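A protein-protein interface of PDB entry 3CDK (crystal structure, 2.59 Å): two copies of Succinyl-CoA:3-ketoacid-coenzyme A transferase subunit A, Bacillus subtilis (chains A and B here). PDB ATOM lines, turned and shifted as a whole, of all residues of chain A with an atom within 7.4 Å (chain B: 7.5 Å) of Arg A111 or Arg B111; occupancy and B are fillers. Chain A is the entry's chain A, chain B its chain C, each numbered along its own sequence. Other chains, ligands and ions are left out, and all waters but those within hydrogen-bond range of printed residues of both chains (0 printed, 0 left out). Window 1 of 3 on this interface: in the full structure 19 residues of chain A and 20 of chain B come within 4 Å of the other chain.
The side-chain carboxylate of Glu A108 is in salt-bridge range of the guanidinium group of Arg B111. OE1 of Glu B108 is in salt-bridge range of NH2 of Arg A111. NH1 of Arg B111 sits close to NH1 of Arg A111 (3.1 Å).
OE2 of Glu A108 is in salt-bridge range of NH1 of Arg A111, 3.2 Å away. The side-chain carboxylate (OE2) of Glu B108 is in salt-bridge range of the guanidinium group (NH1) of Arg B111, 3.3 Å away. The backbone NH (N) of Ile B117 is in hydrogen-bond range of the backbone carbonyl oxygen (O) of Ala B112, 2.8 Å away.
Among the printed residues, pairs that only touch across the chains: Phe A120 with Ile B117 (3.6 Å) and Phe A120 with Phe B120 (3.8 Å).
Of the printed residues of chain B, Glu A108 touches Arg B111 (2.6 Å). Of the printed residues of chain B, Phe A120 touches Ile B117 (3.6 Å) and Phe B120 (3.8 Å). Of the printed residues of chain A, Glu B108 touches Arg A111. Arg B111 touches two residues of chain A. Printed residues of chain A within 4 Å of Ile B117: Phe A120. Of the printed residues of chain A, Phe B120 touches Phe A120 (3.8 Å). The nearest printed residue of chain A that does not touch Ile B117 is Glu A108 (4.6 Å).
Of the 21 printed residues of chain B, 4 touch a printed residue of chain A. Printed residues of chain B that touch a printed residue of chain A: Glu B108, Arg B111, Ile B117 and Phe B120. Hydrophobic or aromatic side chains of chain B that line the printed part of chain A: Ile B117 and Phe B120. Of the 21 printed residues of chain A, 3 touch a printed residue of chain B. Among the printed residues, 5 pairs touch across the chains.
Glu A108 touches Arg B111, and with the chains exchanged Arg A111 touches Glu B108. Arg A111 touches its own counterpart, Arg B111. Phe A120 touches Ile B117, but with the chains exchanged Ile A117 does not touch Phe B120 (4.1 Å). Phe B120 touches its own counterpart, Phe A120. Of the 5 pairs that touch across the chains among the printed residues, 4 have their exchanged pair printed and touching as well.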
ATOM      1  N   THR A 105     -30.422  17.013   5.314  1.00  0.00           N
ATOM      2  CA  THR A 105     -30.489  15.607   5.650  1.00  0.00           C
ATOM      3  C   THR A 105     -29.500  14.790   4.818  1.00  0.00           C
ATOM      4  O   THR A 105     -28.863  13.877   5.340  1.00  0.00           O
ATOM      5  CB  THR A 105     -31.937  15.094   5.527  1.00  0.00           C
ATOM      6  OG1 THR A 105     -32.741  15.715   6.544  1.00  0.00           O
ATOM      7  CG2 THR A 105     -32.010  13.589   5.691  1.00  0.00           C
ATOM      8  N   LEU A 106     -29.356  15.113   3.534  1.00  0.00           N
ATOM      9  CA  LEU A 106     -28.365  14.404   2.716  1.00  0.00           C
ATOM     10  C   LEU A 106     -26.943  14.600   3.217  1.00  0.00           C
ATOM     11  O   LEU A 106     -26.232  13.614   3.404  1.00  0.00           O
ATOM     12  CB  LEU A 106     -28.462  14.801   1.240  1.00  0.00           C
ATOM     13  CG  LEU A 106     -27.558  14.130   0.205  1.00  0.00           C
ATOM     14  CD1 LEU A 106     -27.726  12.629   0.046  1.00  0.00           C
ATOM     15  CD2 LEU A 106     -27.819  14.838  -1.098  1.00  0.00           C
ATOM     16  N   ALA A 107     -26.533  15.844   3.447  1.00  0.00           N
ATOM     17  CA  ALA A 107     -25.232  16.094   4.103  1.00  0.00           C
ATOM     18  C   ALA A 107     -25.064  15.289   5.406  1.00  0.00           C
ATOM     19  O   ALA A 107     -24.106  14.546   5.571  1.00  0.00           O
ATOM     20  CB  ALA A 107     -24.998  17.583   4.347  1.00  0.00           C
ATOM     21  N   GLU A 108     -26.007  15.399   6.324  1.00  0.00           N
ATOM     22  CA  GLU A 108     -25.807  14.755   7.621  1.00  0.00           C
ATOM     23  C   GLU A 108     -25.846  13.231   7.502  1.00  0.00           C
ATOM     24  O   GLU A 108     -25.301  12.522   8.374  1.00  0.00           O
ATOM     25  CB  GLU A 108     -26.779  15.256   8.705  1.00  0.00           C
ATOM     26  CG  GLU A 108     -26.336  14.939  10.127  1.00  0.00           C
ATOM     27  CD  GLU A 108     -25.049  15.693  10.604  1.00  0.00           C
ATOM     28  OE1 GLU A 108     -24.711  16.821  10.124  1.00  0.00           O
ATOM     29  OE2 GLU A 108     -24.364  15.142  11.509  1.00  0.00           O
ATOM     30  N   ARG A 109     -26.458  12.725   6.436  1.00  0.00           N
ATOM     31  CA  ARG A 109     -26.519  11.288   6.280  1.00  0.00           C
ATOM     32  C   ARG A 109     -25.198  10.745   5.818  1.00  0.00           C
ATOM     33  O   ARG A 109     -24.767   9.680   6.279  1.00  0.00           O
ATOM     34  CB  ARG A 109     -27.659  10.839   5.374  1.00  0.00           C
ATOM     35  CG  ARG A 109     -28.987  10.784   6.103  1.00  0.00           C
ATOM     36  CD  ARG A 109     -30.106  10.446   5.118  1.00  0.00           C
ATOM     37  NE  ARG A 109     -29.945   9.097   4.642  1.00  0.00           N
ATOM     38  CZ  ARG A 109     -30.680   8.520   3.696  1.00  0.00           C
ATOM     39  NH1 ARG A 109     -31.650   9.211   3.095  1.00  0.00           N
ATOM     40  NH2 ARG A 109     -30.438   7.228   3.375  1.00  0.00           N
ATOM     41  N   ILE A 110     -24.542  11.483   4.930  1.00  0.00           N
ATOM     42  CA  ILE A 110     -23.255  11.041   4.414  1.00  0.00           C
ATOM     43  C   ILE A 110     -22.260  11.170   5.504  1.00  0.00           C
ATOM     44  O   ILE A 110     -21.473  10.251   5.737  1.00  0.00           O
ATOM     45  CB  ILE A 110     -22.811  11.823   3.175  1.00  0.00           C
ATOM     46  CG1 ILE A 110     -23.814  11.615   2.054  1.00  0.00           C
ATOM     47  CG2 ILE A 110     -21.459  11.346   2.712  1.00  0.00           C
ATOM     48  CD1 ILE A 110     -23.874  12.778   1.203  1.00  0.00           C
ATOM     49  N   ARG A 111     -22.311  12.290   6.217  1.00  0.00           N
ATOM     50  CA  ARG A 111     -21.441  12.420   7.401  1.00  0.00           C
ATOM     51  C   ARG A 111     -21.669  11.226   8.339  1.00  0.00           C
ATOM     52  O   ARG A 111     -20.718  10.572   8.782  1.00  0.00           O
ATOM     53  CB  ARG A 111     -21.691  13.725   8.151  1.00  0.00           C
ATOM     54  CG  ARG A 111     -20.697  13.919   9.276  1.00  0.00           C
ATOM     55  CD  ARG A 111     -20.902  15.186  10.033  1.00  0.00           C
ATOM     56  NE  ARG A 111     -20.059  15.173  11.233  1.00  0.00           N
ATOM     57  CZ  ARG A 111     -20.370  14.554  12.382  1.00  0.00           C
ATOM     58  NH1 ARG A 111     -21.536  13.912  12.528  1.00  0.00           N
ATOM     59  NH2 ARG A 111     -19.518  14.584  13.403  1.00  0.00           N
ATOM     60  N   ALA A 112     -22.940  10.952   8.626  1.00  0.00           N
ATOM     61  CA  ALA A 112     -23.288   9.947   9.601  1.00  0.00           C
ATOM     62  C   ALA A 112     -22.593   8.600   9.261  1.00  0.00           C
ATOM     63  O   ALA A 112     -21.948   7.995  10.115  1.00  0.00           O
ATOM     64  CB  ALA A 112     -24.809   9.814   9.686  1.00  0.00           C
ATOM     65  N   GLY A 113     -22.736   8.166   8.012  1.00  0.00           N
ATOM     66  CA  GLY A 113     -22.256   6.894   7.555  1.00  0.00           C
ATOM     67  C   GLY A 113     -20.748   6.829   7.689  1.00  0.00           C
ATOM     68  O   GLY A 113     -20.191   5.827   8.191  1.00  0.00           O
ATOM     69  N   GLY A 114     -20.099   7.897   7.237  1.00  0.00           N
ATOM     70  CA  GLY A 114     -18.696   8.075   7.484  1.00  0.00           C
ATOM     71  C   GLY A 114     -18.298   8.121   8.944  1.00  0.00           C
ATOM     72  O   GLY A 114     -17.182   7.717   9.296  1.00  0.00           O
ATOM     73  N   ALA A 115     -19.197   8.580   9.803  1.00  0.00           N
ATOM     74  CA  ALA A 115     -18.840   8.782  11.199  1.00  0.00           C
ATOM     75  C   ALA A 115     -19.238   7.615  12.099  1.00  0.00           C
ATOM     76  O   ALA A 115     -19.067   7.672  13.326  1.00  0.00           O
ATOM     77  CB  ALA A 115     -19.442  10.096  11.706  1.00  0.00           C
ATOM     78  N   GLY A 116     -19.768   6.558  11.492  1.00  0.00           N
ATOM     79  CA  GLY A 116     -20.219   5.395  12.236  1.00  0.00           C
ATOM     80  C   GLY A 116     -21.610   5.562  12.828  1.00  0.00           C
ATOM     81  O   GLY A 116     -22.052   4.675  13.541  1.00  0.00           O
ATOM     82  N   ILE A 117     -22.304   6.672  12.565  1.00  0.00           N
ATOM     83  CA  ILE A 117     -23.672   6.855  13.104  1.00  0.00           C
ATOM     84  C   ILE A 117     -24.701   6.166  12.175  1.00  0.00           C
ATOM     85  O   ILE A 117     -24.938   6.651  11.018  1.00  0.00           O
ATOM     86  CB  ILE A 117     -24.129   8.357  13.226  1.00  0.00           C
ATOM     87  CG1 ILE A 117     -23.078   9.330  13.805  1.00  0.00           C
ATOM     88  CG2 ILE A 117     -25.403   8.453  13.945  1.00  0.00           C
ATOM     89  CD1 ILE A 117     -22.178   8.726  14.760  1.00  0.00           C
ATOM     90  N   PHE A 120     -29.871   9.158  13.030  1.00  0.00           N
ATOM     91  CA  PHE A 120     -29.987  10.319  13.904  1.00  0.00           C
ATOM     92  C   PHE A 120     -31.318  10.986  13.589  1.00  0.00           C
ATOM     93  O   PHE A 120     -31.883  10.782  12.517  1.00  0.00           O
ATOM     94  CB  PHE A 120     -28.848  11.337  13.655  1.00  0.00           C
ATOM     95  CG  PHE A 120     -28.880  11.921  12.275  1.00  0.00           C
ATOM     96  CD1 PHE A 120     -28.393  11.189  11.185  1.00  0.00           C
ATOM     97  CD2 PHE A 120     -29.498  13.135  12.039  1.00  0.00           C
ATOM     98  CE1 PHE A 120     -28.476  11.707   9.877  1.00  0.00           C
ATOM     99  CE2 PHE A 120     -29.615  13.662  10.735  1.00  0.00           C
ATOM    100  CZ  PHE A 120     -29.102  12.961   9.651  1.00  0.00           C
ATOM    101  N   GLY A 149     -27.629   6.727   8.309  1.00  0.00           N
ATOM    102  CA  GLY A 149     -26.286   6.958   7.694  1.00  0.00           C
ATOM    103  C   GLY A 149     -26.198   6.332   6.301  1.00  0.00           C
ATOM    104  O   GLY A 149     -26.692   5.215   6.088  1.00  0.00           O
ATOM    105  N   ILE A 150     -25.647   7.074   5.341  1.00  0.00           N
ATOM    106  CA  ILE A 150     -25.345   6.521   4.004  1.00  0.00           C
ATOM    107  C   ILE A 150     -23.860   6.227   3.842  1.00  0.00           C
ATOM    108  O   ILE A 150     -23.001   7.028   4.209  1.00  0.00           O
ATOM    109  CB  ILE A 150     -25.698   7.479   2.860  1.00  0.00           C
ATOM    110  CG1 ILE A 150     -27.202   7.750   2.795  1.00  0.00           C
ATOM    111  CG2 ILE A 150     -25.153   6.922   1.496  1.00  0.00           C
ATOM    112  CD1 ILE A 150     -27.560   8.938   1.925  1.00  0.00           C
ATOM    113  N   PRO A 179     -15.748  17.059   1.481  1.00  0.00           N
ATOM    114  CA  PRO A 179     -15.135  16.504   2.690  1.00  0.00           C
ATOM    115  C   PRO A 179     -15.979  15.424   3.323  1.00  0.00           C
ATOM    116  O   PRO A 179     -15.461  14.441   3.848  1.00  0.00           O
ATOM    117  CB  PRO A 179     -15.058  17.709   3.660  1.00  0.00           C
ATOM    118  CG  PRO A 179     -15.335  18.886   2.876  1.00  0.00           C
ATOM    119  CD  PRO A 179     -16.121  18.470   1.663  1.00  0.00           C
ATOM    120  N   ILE A 180     -17.282  15.612   3.300  1.00  0.00           N
ATOM    121  CA  ILE A 180     -18.124  14.662   3.988  1.00  0.00           C
ATOM    122  C   ILE A 180     -18.237  13.391   3.172  1.00  0.00           C
ATOM    123  O   ILE A 180     -18.287  12.293   3.747  1.00  0.00           O
ATOM    124  CB  ILE A 180     -19.470  15.298   4.423  1.00  0.00           C
ATOM    125  CG1 ILE A 180     -20.160  16.019   3.288  1.00  0.00           C
ATOM    126  CG2 ILE A 180     -19.204  16.357   5.538  1.00  0.00           C
ATOM    127  CD1 ILE A 180     -21.634  16.234   3.589  1.00  0.00           C
ATOM    128  N   ALA A 181     -18.207  13.540   1.838  1.00  0.00           N
ATOM    129  CA  ALA A 181     -18.192  12.392   0.956  1.00  0.00           C
ATOM    130  C   ALA A 181     -16.874  11.604   1.100  1.00  0.00           C
ATOM    131  O   ALA A 181     -16.879  10.355   1.129  1.00  0.00           O
ATOM    132  CB  ALA A 181     -18.412  12.812  -0.493  1.00  0.00           C
ATOM    133  N   MET A 183     -15.254  10.946   3.588  1.00  0.00           N
ATOM    134  CA  MET A 183     -15.439  10.081   4.767  1.00  0.00           C
ATOM    135  C   MET A 183     -16.279   8.820   4.558  1.00  0.00           C
ATOM    136  O   MET A 183     -15.996   7.777   5.128  1.00  0.00           O
ATOM    137  CB  MET A 183     -16.167  10.851   5.895  1.00  0.00           C
ATOM    138  CG  MET A 183     -15.481  12.054   6.516  1.00  0.00           C
ATOM    139  SD  MET A 183     -16.808  12.994   7.355  1.00  0.00           S
ATOM    140  CE  MET A 183     -16.262  14.726   7.201  1.00  0.00           C
ATOM    141  N   ALA A 184     -17.376   8.954   3.833  1.00  0.00           N
ATOM    142  CA  ALA A 184     -18.351   7.880   3.661  1.00  0.00           C
ATOM    143  C   ALA A 184     -17.980   6.843   2.619  1.00  0.00           C
ATOM    144  O   ALA A 184     -18.751   5.938   2.372  1.00  0.00           O
ATOM    145  CB  ALA A 184     -19.720   8.477   3.307  1.00  0.00           C
ATOM    146  N   THR B 105     -18.708   9.842  22.385  1.00  0.00           N
ATOM    147  CA  THR B 105     -20.118  10.106  22.533  1.00  0.00           C
ATOM    148  C   THR B 105     -20.325  11.492  23.034  1.00  0.00           C
ATOM    149  O   THR B 105     -21.330  12.126  22.727  1.00  0.00           O
ATOM    150  CB  THR B 105     -20.784   9.161  23.523  1.00  0.00           C
ATOM    151  OG1 THR B 105     -20.855   7.839  22.963  1.00  0.00           O
ATOM    152  CG2 THR B 105     -22.203   9.670  23.880  1.00  0.00           C
ATOM    153  N   LEU B 106     -19.383  11.959  23.842  1.00  0.00           N
ATOM    154  CA  LEU B 106     -19.495  13.251  24.472  1.00  0.00           C
ATOM    155  C   LEU B 106     -19.381  14.308  23.393  1.00  0.00           C
ATOM    156  O   LEU B 106     -20.259  15.173  23.277  1.00  0.00           O
ATOM    157  CB  LEU B 106     -18.415  13.412  25.523  1.00  0.00           C
ATOM    158  CG  LEU B 106     -18.362  14.770  26.233  1.00  0.00           C
ATOM    159  CD1 LEU B 106     -19.751  15.170  26.736  1.00  0.00           C
ATOM    160  CD2 LEU B 106     -17.341  14.803  27.363  1.00  0.00           C
ATOM    161  N   ALA B 107     -18.304  14.230  22.617  1.00  0.00           N
ATOM    162  CA  ALA B 107     -18.062  15.117  21.461  1.00  0.00           C
ATOM    163  C   ALA B 107     -19.281  15.195  20.558  1.00  0.00           C
ATOM    164  O   ALA B 107     -19.774  16.280  20.206  1.00  0.00           O
ATOM    165  CB  ALA B 107     -16.851  14.601  20.639  1.00  0.00           C
ATOM    166  N   GLU B 108     -19.796  14.024  20.200  1.00  0.00           N
ATOM    167  CA  GLU B 108     -20.874  13.968  19.239  1.00  0.00           C
ATOM    168  C   GLU B 108     -22.180  14.504  19.881  1.00  0.00           C
ATOM    169  O   GLU B 108     -22.987  15.134  19.188  1.00  0.00           O
ATOM    170  CB  GLU B 108     -20.968  12.535  18.697  1.00  0.00           C
ATOM    171  CG  GLU B 108     -21.687  12.319  17.380  1.00  0.00           C
ATOM    172  CD  GLU B 108     -21.278  13.268  16.226  1.00  0.00           C
ATOM    173  OE1 GLU B 108     -20.072  13.507  16.008  1.00  0.00           O
ATOM    174  OE2 GLU B 108     -22.176  13.749  15.495  1.00  0.00           O
ATOM    175  N   ARG B 109     -22.382  14.282  21.183  1.00  0.00           N
ATOM    176  CA  ARG B 109     -23.592  14.797  21.863  1.00  0.00           C
ATOM    177  C   ARG B 109     -23.598  16.304  21.827  1.00  0.00           C
ATOM    178  O   ARG B 109     -24.622  16.903  21.497  1.00  0.00           O
ATOM    179  CB  ARG B 109     -23.721  14.317  23.312  1.00  0.00           C
ATOM    180  CG  ARG B 109     -24.201  12.860  23.420  1.00  0.00           C
ATOM    181  CD  ARG B 109     -24.242  12.346  24.859  1.00  0.00           C
ATOM    182  NE  ARG B 109     -25.315  13.017  25.546  1.00  0.00           N
ATOM    183  CZ  ARG B 109     -25.557  12.992  26.850  1.00  0.00           C
ATOM    184  NH1 ARG B 109     -24.782  12.264  27.670  1.00  0.00           N
ATOM    185  NH2 ARG B 109     -26.616  13.696  27.320  1.00  0.00           N
ATOM    186  N   ILE B 110     -22.445  16.908  22.155  1.00  0.00           N
ATOM    187  CA  ILE B 110     -22.291  18.362  22.115  1.00  0.00           C
ATOM    188  C   ILE B 110     -22.465  18.830  20.675  1.00  0.00           C
ATOM    189  O   ILE B 110     -23.214  19.773  20.410  1.00  0.00           O
ATOM    190  CB  ILE B 110     -20.938  18.814  22.714  1.00  0.00           C
ATOM    191  CG1 ILE B 110     -20.908  18.473  24.205  1.00  0.00           C
ATOM    192  CG2 ILE B 110     -20.661  20.318  22.439  1.00  0.00           C
ATOM    193  CD1 ILE B 110     -19.545  18.462  24.819  1.00  0.00           C
ATOM    194  N   ARG B 111     -21.844  18.147  19.719  1.00  0.00           N
ATOM    195  CA  ARG B 111     -22.037  18.587  18.334  1.00  0.00           C
ATOM    196  C   ARG B 111     -23.514  18.542  17.926  1.00  0.00           C
ATOM    197  O   ARG B 111     -23.973  19.413  17.195  1.00  0.00           O
ATOM    198  CB  ARG B 111     -21.184  17.809  17.344  1.00  0.00           C
ATOM    199  CG  ARG B 111     -21.541  18.202  15.925  1.00  0.00           C
ATOM    200  CD  ARG B 111     -20.846  17.398  14.872  1.00  0.00           C
ATOM    201  NE  ARG B 111     -21.354  17.742  13.539  1.00  0.00           N
ATOM    202  CZ  ARG B 111     -22.428  17.204  12.948  1.00  0.00           C
ATOM    203  NH1 ARG B 111     -23.158  16.285  13.563  1.00  0.00           N
ATOM    204  NH2 ARG B 111     -22.768  17.591  11.722  1.00  0.00           N
ATOM    205  N   ALA B 112     -24.243  17.528  18.410  1.00  0.00           N
ATOM    206  CA  ALA B 112     -25.645  17.355  18.067  1.00  0.00           C
ATOM    207  C   ALA B 112     -26.490  18.486  18.633  1.00  0.00           C
ATOM    208  O   ALA B 112     -27.406  18.962  17.981  1.00  0.00           O
ATOM    209  CB  ALA B 112     -26.131  16.037  18.577  1.00  0.00           C
ATOM    210  N   GLY B 113     -26.190  18.909  19.857  1.00  0.00           N
ATOM    211  CA  GLY B 113     -26.906  19.999  20.484  1.00  0.00           C
ATOM    212  C   GLY B 113     -26.799  21.196  19.550  1.00  0.00           C
ATOM    213  O   GLY B 113     -27.829  21.838  19.181  1.00  0.00           O
ATOM    214  N   GLY B 114     -25.577  21.474  19.113  1.00  0.00           N
ATOM    215  CA  GLY B 114     -25.376  22.639  18.308  1.00  0.00           C
ATOM    216  C   GLY B 114     -25.917  22.485  16.902  1.00  0.00           C
ATOM    217  O   GLY B 114     -26.281  23.483  16.272  1.00  0.00           O
ATOM    218  N   ALA B 115     -25.990  21.239  16.431  1.00  0.00           N
ATOM    219  CA  ALA B 115     -26.410  20.937  15.061  1.00  0.00           C
ATOM    220  C   ALA B 115     -27.914  20.629  14.943  1.00  0.00           C
ATOM    221  O   ALA B 115     -28.409  20.272  13.847  1.00  0.00           O
ATOM    222  CB  ALA B 115     -25.574  19.788  14.476  1.00  0.00           C
ATOM    223  N   GLY B 116     -28.630  20.791  16.069  1.00  0.00           N
ATOM    224  CA  GLY B 116     -30.065  20.544  16.143  1.00  0.00           C
ATOM    225  C   GLY B 116     -30.454  19.075  16.192  1.00  0.00           C
ATOM    226  O   GLY B 116     -31.623  18.765  16.121  1.00  0.00           O
ATOM    227  N   ILE B 117     -29.476  18.167  16.283  1.00  0.00           N
ATOM    228  CA  ILE B 117     -29.740  16.741  16.473  1.00  0.00           C
ATOM    229  C   ILE B 117     -30.145  16.451  17.930  1.00  0.00           C
ATOM    230  O   ILE B 117     -29.326  16.527  18.837  1.00  0.00           O
ATOM    231  CB  ILE B 117     -28.502  15.884  16.104  1.00  0.00           C
ATOM    232  CG1 ILE B 117     -27.902  16.249  14.725  1.00  0.00           C
ATOM    233  CG2 ILE B 117     -28.808  14.428  16.185  1.00  0.00           C
ATOM    234  CD1 ILE B 117     -28.884  16.344  13.651  1.00  0.00           C
ATOM    235  N   PHE B 120     -29.087  10.513  18.460  1.00  0.00           N
ATOM    236  CA  PHE B 120     -28.302   9.836  17.425  1.00  0.00           C
ATOM    237  C   PHE B 120     -27.779   8.537  18.002  1.00  0.00           C
ATOM    238  O   PHE B 120     -27.591   8.412  19.219  1.00  0.00           O
ATOM    239  CB  PHE B 120     -27.122  10.699  16.954  1.00  0.00           C
ATOM    240  CG  PHE B 120     -25.995  10.778  17.956  1.00  0.00           C
ATOM    241  CD1 PHE B 120     -25.986  11.785  18.954  1.00  0.00           C
ATOM    242  CD2 PHE B 120     -24.969   9.821  17.954  1.00  0.00           C
ATOM    243  CE1 PHE B 120     -24.944  11.842  19.917  1.00  0.00           C
ATOM    244  CE2 PHE B 120     -23.932   9.875  18.920  1.00  0.00           C
ATOM    245  CZ  PHE B 120     -23.910  10.886  19.893  1.00  0.00           C
ATOM    246  N   GLY B 149     -28.544  14.882  22.296  1.00  0.00           N
ATOM    247  CA  GLY B 149     -27.919  16.213  22.072  1.00  0.00           C
ATOM    248  C   GLY B 149     -27.755  16.981  23.369  1.00  0.00           C
ATOM    249  O   GLY B 149     -28.670  16.952  24.210  1.00  0.00           O
ATOM    250  N   ILE B 150     -26.594  17.630  23.572  1.00  0.00           N
ATOM    251  CA  ILE B 150     -26.358  18.509  24.767  1.00  0.00           C
ATOM    252  C   ILE B 150     -26.325  20.004  24.429  1.00  0.00           C
ATOM    253  O   ILE B 150     -25.707  20.404  23.464  1.00  0.00           O
ATOM    254  CB  ILE B 150     -25.064  18.181  25.498  1.00  0.00           C
ATOM    255  CG1 ILE B 150     -25.207  16.868  26.260  1.00  0.00           C
ATOM    256  CG2 ILE B 150     -24.692  19.305  26.455  1.00  0.00           C
ATOM    257  CD1 ILE B 150     -23.855  16.041  26.312  1.00  0.00           C
ATOM    258  N   PRO B 179     -14.372  24.051  18.960  1.00  0.00           N
ATOM    259  CA  PRO B 179     -15.321  24.335  17.863  1.00  0.00           C
ATOM    260  C   PRO B 179     -16.714  23.831  18.158  1.00  0.00           C
ATOM    261  O   PRO B 179     -17.690  24.486  17.825  1.00  0.00           O
ATOM    262  CB  PRO B 179     -14.753  23.552  16.652  1.00  0.00           C
ATOM    263  CG  PRO B 179     -13.382  23.263  16.972  1.00  0.00           C
ATOM    264  CD  PRO B 179     -13.205  23.281  18.484  1.00  0.00           C
ATOM    265  N   ILE B 180     -16.808  22.662  18.765  1.00  0.00           N
ATOM    266  CA  ILE B 180     -18.130  22.086  18.997  1.00  0.00           C
ATOM    267  C   ILE B 180     -18.811  22.692  20.191  1.00  0.00           C
ATOM    268  O   ILE B 180     -20.026  22.913  20.151  1.00  0.00           O
ATOM    269  CB  ILE B 180     -18.159  20.524  19.007  1.00  0.00           C
ATOM    270  CG1 ILE B 180     -17.234  19.938  20.064  1.00  0.00           C
ATOM    271  CG2 ILE B 180     -17.801  19.969  17.568  1.00  0.00           C
ATOM    272  CD1 ILE B 180     -17.273  18.407  20.075  1.00  0.00           C
ATOM    273  N   ALA B 181     -18.026  23.035  21.224  1.00  0.00           N
ATOM    274  CA  ALA B 181     -18.602  23.635  22.424  1.00  0.00           C
ATOM    275  C   ALA B 181     -19.192  25.006  22.064  1.00  0.00           C
ATOM    276  O   ALA B 181     -20.272  25.405  22.552  1.00  0.00           O
ATOM    277  CB  ALA B 181     -17.605  23.730  23.477  1.00  0.00           C
ATOM    278  N   MET B 183     -20.714  25.693  19.352  1.00  0.00           N
ATOM    279  CA  MET B 183     -22.053  25.548  18.730  1.00  0.00           C
ATOM    280  C   MET B 183     -23.178  25.321  19.712  1.00  0.00           C
ATOM    281  O   MET B 183     -24.320  25.691  19.461  1.00  0.00           O
ATOM    282  CB  MET B 183     -22.126  24.362  17.765  1.00  0.00           C
ATOM    283  CG  MET B 183     -21.219  24.389  16.599  1.00  0.00           C
ATOM    284  SD  MET B 183     -21.039  22.677  16.069  1.00  0.00           S
ATOM    285  CE  MET B 183     -19.487  22.902  15.163  1.00  0.00           C
ATOM    286  N   ALA B 184     -22.859  24.632  20.791  1.00  0.00           N
ATOM    287  CA  ALA B 184     -23.863  24.210  21.771  1.00  0.00           C
ATOM    288  C   ALA B 184     -24.288  25.281  22.794  1.00  0.00           C
ATOM    289  O   ALA B 184     -25.360  25.166  23.387  1.00  0.00           O
ATOM    290  CB  ALA B 184     -23.463  22.884  22.451  1.00  0.00           C
